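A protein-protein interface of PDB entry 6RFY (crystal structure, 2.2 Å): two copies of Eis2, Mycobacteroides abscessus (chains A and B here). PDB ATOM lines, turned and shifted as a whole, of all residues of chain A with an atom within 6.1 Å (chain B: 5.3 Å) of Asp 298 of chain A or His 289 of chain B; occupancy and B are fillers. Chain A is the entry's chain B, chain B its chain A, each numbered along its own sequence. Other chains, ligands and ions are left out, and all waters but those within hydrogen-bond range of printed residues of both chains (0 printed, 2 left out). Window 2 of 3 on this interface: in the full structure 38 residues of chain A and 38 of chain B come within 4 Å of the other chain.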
ATOM      1  N   ALA A 118      22.844   9.922 -12.919  1.00  0.00           N
ATOM      2  CA  ALA A 118      23.598   8.809 -12.355  1.00  0.00           C
ATOM      3  C   ALA A 118      24.540   9.240 -11.237  1.00  0.00           C
ATOM      4  O   ALA A 118      24.928   8.405 -10.413  1.00  0.00           O
ATOM      5  CB  ALA A 118      24.389   8.102 -13.455  1.00  0.00           C
ATOM      6  N   SER A 119      24.916  10.521 -11.187  1.00  0.00           N
ATOM      7  CA  SER A 119      25.782  11.018 -10.123  1.00  0.00           C
ATOM      8  C   SER A 119      25.112  10.998  -8.753  1.00  0.00           C
ATOM      9  O   SER A 119      25.780  11.281  -7.752  1.00  0.00           O
ATOM     10  CB  SER A 119      26.252  12.439 -10.448  1.00  0.00           C
ATOM     11  OG  SER A 119      25.151  13.318 -10.597  1.00  0.00           O
ATOM     12  N   TYR A 124      22.055   4.558  -7.000  1.00  0.00           N
ATOM     13  CA  TYR A 124      22.397   4.112  -8.350  1.00  0.00           C
ATOM     14  C   TYR A 124      21.863   2.708  -8.622  1.00  0.00           C
ATOM     15  O   TYR A 124      22.163   1.764  -7.883  1.00  0.00           O
ATOM     16  CB  TYR A 124      23.914   4.152  -8.548  1.00  0.00           C
ATOM     17  CG  TYR A 124      24.360   3.704  -9.927  1.00  0.00           C
ATOM     18  CD1 TYR A 124      24.619   2.365 -10.202  1.00  0.00           C
ATOM     19  CD2 TYR A 124      24.519   4.624 -10.955  1.00  0.00           C
ATOM     20  CE1 TYR A 124      25.018   1.957 -11.460  1.00  0.00           C
ATOM     21  CE2 TYR A 124      24.921   4.225 -12.218  1.00  0.00           C
ATOM     22  CZ  TYR A 124      25.169   2.891 -12.464  1.00  0.00           C
ATOM     23  OH  TYR A 124      25.570   2.491 -13.720  1.00  0.00           O
ATOM     24  N   VAL A 131      19.795   3.084 -16.553  1.00  0.00           N
ATOM     25  CA  VAL A 131      20.556   4.070 -17.314  1.00  0.00           C
ATOM     26  C   VAL A 131      20.078   4.050 -18.760  1.00  0.00           C
ATOM     27  O   VAL A 131      20.184   3.030 -19.452  1.00  0.00           O
ATOM     28  CB  VAL A 131      22.064   3.797 -17.225  1.00  0.00           C
ATOM     29  CG1 VAL A 131      22.818   4.720 -18.172  1.00  0.00           C
ATOM     30  CG2 VAL A 131      22.560   3.979 -15.797  1.00  0.00           C
ATOM     31  N   THR A 133      20.558   7.175 -20.878  1.00  0.00           N
ATOM     32  CA  THR A 133      21.273   8.194 -21.627  1.00  0.00           C
ATOM     33  C   THR A 133      22.712   8.242 -21.136  1.00  0.00           C
ATOM     34  O   THR A 133      22.973   8.102 -19.937  1.00  0.00           O
ATOM     35  CB  THR A 133      20.609   9.574 -21.461  1.00  0.00           C
ATOM     36  OG1 THR A 133      19.267   9.521 -21.959  1.00  0.00           O
ATOM     37  CG2 THR A 133      21.373  10.646 -22.221  1.00  0.00           C
ATOM     38  N   GLU A 134      23.641   8.426 -22.069  1.00  0.00           N
ATOM     39  CA  GLU A 134      25.048   8.588 -21.753  1.00  0.00           C
ATOM     40  C   GLU A 134      25.507   9.983 -22.152  1.00  0.00           C
ATOM     41  O   GLU A 134      24.846  10.684 -22.922  1.00  0.00           O
ATOM     42  CB  GLU A 134      25.913   7.540 -22.465  1.00  0.00           C
ATOM     43  CG  GLU A 134      25.524   6.108 -22.180  1.00  0.00           C
ATOM     44  CD  GLU A 134      26.419   5.120 -22.899  1.00  0.00           C
ATOM     45  OE1 GLU A 134      27.194   4.419 -22.217  1.00  0.00           O
ATOM     46  OE2 GLU A 134      26.364   5.061 -24.146  1.00  0.00           O
ATOM     47  N   SER A 135      26.654  10.381 -21.610  1.00  0.00           N
ATOM     48  CA  SER A 135      27.306  11.623 -21.983  1.00  0.00           C
ATOM     49  C   SER A 135      28.765  11.335 -22.299  1.00  0.00           C
ATOM     50  O   SER A 135      29.327  10.322 -21.879  1.00  0.00           O
ATOM     51  CB  SER A 135      27.199  12.687 -20.880  1.00  0.00           C
ATOM     52  OG  SER A 135      27.817  12.254 -19.683  1.00  0.00           O
ATOM     53  N   VAL A 296      33.028   7.971 -22.522  1.00  0.00           N
ATOM     54  CA  VAL A 296      31.584   7.791 -22.408  1.00  0.00           C
ATOM     55  C   VAL A 296      31.246   7.301 -21.008  1.00  0.00           C
ATOM     56  O   VAL A 296      31.898   6.392 -20.482  1.00  0.00           O
ATOM     57  CB  VAL A 296      31.064   6.805 -23.476  1.00  0.00           C
ATOM     58  CG1 VAL A 296      29.573   6.555 -23.299  1.00  0.00           C
ATOM     59  CG2 VAL A 296      31.347   7.338 -24.871  1.00  0.00           C
ATOM     60  N   SER A 297      30.213   7.888 -20.405  1.00  0.00           N
ATOM     61  CA  SER A 297      29.790   7.492 -19.068  1.00  0.00           C
ATOM     62  C   SER A 297      28.286   7.692 -18.933  1.00  0.00           C
ATOM     63  O   SER A 297      27.644   8.318 -19.781  1.00  0.00           O
ATOM     64  CB  SER A 297      30.545   8.279 -17.991  1.00  0.00           C
ATOM     65  OG  SER A 297      30.426   9.675 -18.204  1.00  0.00           O
ATOM     66  N   ASP A 298      27.730   7.153 -17.846  1.00  0.00           N
ATOM     67  CA  ASP A 298      26.303   7.289 -17.579  1.00  0.00           C
ATOM     68  C   ASP A 298      25.901   8.751 -17.438  1.00  0.00           C
ATOM     69  O   ASP A 298      26.657   9.582 -16.929  1.00  0.00           O
ATOM     70  CB  ASP A 298      25.912   6.557 -16.296  1.00  0.00           C
ATOM     71  CG  ASP A 298      26.085   5.063 -16.387  1.00  0.00           C
ATOM     72  OD1 ASP A 298      26.130   4.524 -17.515  1.00  0.00           O
ATOM     73  OD2 ASP A 298      26.148   4.427 -15.314  1.00  0.00           O
ATOM     74  N   ALA A 299      24.670   9.049 -17.859  1.00  0.00           N
ATOM     75  CA  ALA A 299      24.102  10.377 -17.668  1.00  0.00           C
ATOM     76  C   ALA A 299      22.782  10.313 -16.905  1.00  0.00           C
ATOM     77  O   ALA A 299      22.741  10.631 -15.712  1.00  0.00           O
ATOM     78  CB  ALA A 299      23.903  11.078 -19.012  1.00  0.00           C
ATOM     79  N   ILE A 300      21.705   9.898 -17.573  1.00  0.00           N
ATOM     80  CA  ILE A 300      20.356   9.959 -17.016  1.00  0.00           C
ATOM     81  C   ILE A 300      19.807   8.549 -16.847  1.00  0.00           C
ATOM     82  O   ILE A 300      19.921   7.717 -17.754  1.00  0.00           O
ATOM     83  CB  ILE A 300      19.418  10.801 -17.903  1.00  0.00           C
ATOM     84  CG1 ILE A 300      19.779  12.283 -17.796  1.00  0.00           C
ATOM     85  CG2 ILE A 300      17.954  10.567 -17.526  1.00  0.00           C
ATOM     86  CD1 ILE A 300      19.431  12.904 -16.461  1.00  0.00           C
ATOM     87  N   ARG B 283      30.094  -4.229 -20.682  1.00  0.00           N
ATOM     88  CA  ARG B 283      29.682  -2.919 -20.186  1.00  0.00           C
ATOM     89  C   ARG B 283      28.335  -2.976 -19.481  1.00  0.00           C
ATOM     90  O   ARG B 283      28.082  -2.189 -18.562  1.00  0.00           O
ATOM     91  CB  ARG B 283      29.621  -1.909 -21.333  1.00  0.00           C
ATOM     92  CG  ARG B 283      30.941  -1.670 -22.045  1.00  0.00           C
ATOM     93  CD  ARG B 283      30.813  -0.511 -23.024  1.00  0.00           C
ATOM     94  NE  ARG B 283      30.500   0.734 -22.326  1.00  0.00           N
ATOM     95  CZ  ARG B 283      29.881   1.770 -22.883  1.00  0.00           C
ATOM     96  NH1 ARG B 283      29.499   1.713 -24.152  1.00  0.00           N
ATOM     97  NH2 ARG B 283      29.636   2.860 -22.167  1.00  0.00           N
ATOM     98  N   TYR B 284      27.455  -3.880 -19.902  1.00  0.00           N
ATOM     99  CA  TYR B 284      26.114  -3.989 -19.345  1.00  0.00           C
ATOM    100  C   TYR B 284      25.993  -5.104 -18.316  1.00  0.00           C
ATOM    101  O   TYR B 284      24.981  -5.164 -17.610  1.00  0.00           O
ATOM    102  CB  TYR B 284      25.097  -4.183 -20.478  1.00  0.00           C
ATOM    103  CG  TYR B 284      25.277  -3.136 -21.555  1.00  0.00           C
ATOM    104  CD1 TYR B 284      24.675  -1.888 -21.447  1.00  0.00           C
ATOM    105  CD2 TYR B 284      26.100  -3.374 -22.646  1.00  0.00           C
ATOM    106  CE1 TYR B 284      24.863  -0.919 -22.416  1.00  0.00           C
ATOM    107  CE2 TYR B 284      26.297  -2.413 -23.616  1.00  0.00           C
ATOM    108  CZ  TYR B 284      25.676  -1.189 -23.499  1.00  0.00           C
ATOM    109  OH  TYR B 284      25.873  -0.236 -24.470  1.00  0.00           O
ATOM    110  N   VAL B 286      28.351  -5.331 -15.879  1.00  0.00           N
ATOM    111  CA  VAL B 286      28.833  -4.664 -14.675  1.00  0.00           C
ATOM    112  C   VAL B 286      27.690  -3.916 -14.005  1.00  0.00           C
ATOM    113  O   VAL B 286      26.922  -3.198 -14.659  1.00  0.00           O
ATOM    114  CB  VAL B 286      29.995  -3.720 -15.020  1.00  0.00           C
ATOM    115  CG1 VAL B 286      30.333  -2.831 -13.833  1.00  0.00           C
ATOM    116  CG2 VAL B 286      31.214  -4.518 -15.453  1.00  0.00           C
ATOM    117  N   ALA B 287      27.570  -4.085 -12.686  1.00  0.00           N
ATOM    118  CA  ALA B 287      26.470  -3.462 -11.956  1.00  0.00           C
ATOM    119  C   ALA B 287      26.646  -1.952 -11.870  1.00  0.00           C
ATOM    120  O   ALA B 287      25.664  -1.202 -11.935  1.00  0.00           O
ATOM    121  CB  ALA B 287      26.356  -4.067 -10.558  1.00  0.00           C
ATOM    122  N   ASN B 288      27.882  -1.488 -11.712  1.00  0.00           N
ATOM    123  CA  ASN B 288      28.186  -0.073 -11.522  1.00  0.00           C
ATOM    124  C   ASN B 288      29.017   0.403 -12.712  1.00  0.00           C
ATOM    125  O   ASN B 288      30.249   0.317 -12.690  1.00  0.00           O
ATOM    126  CB  ASN B 288      28.911   0.144 -10.196  1.00  0.00           C
ATOM    127  CG  ASN B 288      29.105   1.607  -9.871  1.00  0.00           C
ATOM    128  OD1 ASN B 288      30.199   2.148 -10.032  1.00  0.00           O
ATOM    129  ND2 ASN B 288      28.044   2.259  -9.410  1.00  0.00           N
ATOM    130  N   HIS B 289      28.337   0.906 -13.743  1.00  0.00           N
ATOM    131  CA  HIS B 289      29.020   1.373 -14.947  1.00  0.00           C
ATOM    132  C   HIS B 289      30.181   2.329 -14.678  1.00  0.00           C
ATOM    133  O   HIS B 289      31.214   2.192 -15.356  1.00  0.00           O
ATOM    134  CB  HIS B 289      28.021   2.054 -15.898  1.00  0.00           C
ATOM    135  CG  HIS B 289      26.942   1.151 -16.413  1.00  0.00           C
ATOM    136  ND1 HIS B 289      25.848   1.627 -17.104  1.00  0.00           N
ATOM    137  CD2 HIS B 289      26.790  -0.193 -16.349  1.00  0.00           C
ATOM    138  CE1 HIS B 289      25.064   0.617 -17.434  1.00  0.00           C
ATOM    139  NE2 HIS B 289      25.613  -0.499 -16.989  1.00  0.00           N
ATOM    140  N   PRO B 290      30.092   3.304 -13.761  1.00  0.00           N
ATOM    141  CA  PRO B 290      31.234   4.219 -13.566  1.00  0.00           C
ATOM    142  C   PRO B 290      32.534   3.530 -13.183  1.00  0.00           C
ATOM    143  O   PRO B 290      33.602   4.142 -13.320  1.00  0.00           O
ATOM    144  CB  PRO B 290      30.749   5.151 -12.448  1.00  0.00           C
ATOM    145  CG  PRO B 290      29.270   5.155 -12.586  1.00  0.00           C
ATOM    146  CD  PRO B 290      28.908   3.758 -13.005  1.00  0.00           C
ATOM    147  N   SER B 291      32.489   2.288 -12.702  1.00  0.00           N
ATOM    148  CA  SER B 291      33.716   1.575 -12.371  1.00  0.00           C
ATOM    149  C   SER B 291      34.450   1.065 -13.604  1.00  0.00           C
ATOM    150  O   SER B 291      35.639   0.744 -13.509  1.00  0.00           O
ATOM    151  CB  SER B 291      33.408   0.406 -11.432  1.00  0.00           C
ATOM    152  OG  SER B 291      32.890   0.874 -10.198  1.00  0.00           O
ATOM    153  N   LEU B 292      33.782   0.998 -14.754  1.00  0.00           N
ATOM    154  CA  LEU B 292      34.378   0.516 -15.998  1.00  0.00           C
ATOM    155  C   LEU B 292      34.516   1.695 -16.956  1.00  0.00           C
ATOM    156  O   LEU B 292      33.542   2.107 -17.594  1.00  0.00           O
ATOM    157  CB  LEU B 292      33.533  -0.603 -16.601  1.00  0.00           C
ATOM    158  CG  LEU B 292      34.128  -1.350 -17.798  1.00  0.00           C
ATOM    159  CD1 LEU B 292      35.379  -2.121 -17.392  1.00  0.00           C
ATOM    160  CD2 LEU B 292      33.093  -2.278 -18.420  1.00  0.00           C
ATOM    161  N   GLU B 293      35.724   2.246 -17.045  1.00  0.00           N
ATOM    162  CA  GLU B 293      35.965   3.363 -17.945  1.00  0.00           C
ATOM    163  C   GLU B 293      35.853   2.912 -19.394  1.00  0.00           C
ATOM    164  O   GLU B 293      36.280   1.813 -19.757  1.00  0.00           O
ATOM    165  CB  GLU B 293      37.344   3.973 -17.702  1.00  0.00           C
ATOM    166  CG  GLU B 293      37.539   5.300 -18.425  1.00  0.00           C
ATOM    167  CD  GLU B 293      38.964   5.804 -18.364  1.00  0.00           C
ATOM    168  OE1 GLU B 293      39.879   5.040 -18.737  1.00  0.00           O
ATOM    169  OE2 GLU B 293      39.167   6.969 -17.958  1.00  0.00           O
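The side-chain carboxylate of Glu 134 of chain A is in salt-bridge range of the guanidinium group of Arg 283 of chain B (2.9 Å). The backbone NH of His 289 of chain B lies within hydrogen-bond range of the side-chain hydroxyl of Tyr 124 of chain A, 3.2 Å away. A ring nitrogen (ND1) of His 289 of chain B lies within hydrogen-bond range of the side-chain carboxylate of Asp 298 of chain A, 2.9 Å away.
O of Arg 283 of chain B sits close to NE2 of His 289 of chain B (3.4 Å). The side-chain amide oxygen (OD1) of Asn 288 of chain B sits at hydrogen-bond distance from the side-chain hydroxyl (OG) of Ser 291 of chain B, at 3.0 Å. OH of Tyr 124 of chain A sits at hydrogen-bond distance from OD2 of Asp 298 of chain A (2.6 Å).
Tyr 124 of chain A touches Ala 287 of chain B (CE1 to O, 3.3 Å). ND2 of Asn 288 of chain B touches CD1 of Tyr 124 of chain A, 3.5 Å away. OH of Tyr 124 of chain A touches CD of Pro 290 of chain B, 3.6 Å away. NH2 of Arg 283 of chain B touches CG1 of Val 296 of chain A, at 3.9 Å. Pro 290 of chain B touches Asp 298 of chain A (CD to OD2, 3.7 Å).
Asp 298 of chain A touches two residues of chain B. His 289 of chain B touches just these residues of chain A: Tyr 124 and Asp 298. Of the printed residues of chain B, Tyr 124 of chain A touches Ala 287, Asn 288, His 289 and Pro 290. Of the printed residues of chain A, Arg 283 of chain B touches Glu 134 and Val 296. Of the printed residues of chain A, Asn 288 of chain B touches Tyr 124 (3.5 Å). Of the printed residues of chain B, Glu 134 of chain A touches Arg 283. Ser 291 of chain B touches none of the printed residues of chain A. The nearest printed residue of chain B that does not touch Asp 298 of chain A is Asn 288 of chain B (5.6 Å). The nearest printed residue of chain B that does not touch Tyr 124 of chain A is Val 286 of chain B (5.9 Å).
Printed residues of chain B that touch a printed residue of chain A: Arg 283, Ala 287, Asn 288, His 289 and Pro 290. Hydrophobic or aromatic side chains of chain B within 4 Å of the printed part of chain A: His 289 and Pro 290. Along chain B the printed residues that touch a printed residue of chain A span positions 283 to 290. Of the 12 printed residues of chain A, 4 touch a printed residue of chain B. Printed residues of chain A that touch a printed residue of chain B: Tyr 124, Glu 134, Val 296 and Asp 298. Hydrophobic or aromatic side chains of chain A that line the printed part of chain B: Tyr 124 and Val 296.
No position is printed for both chains.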
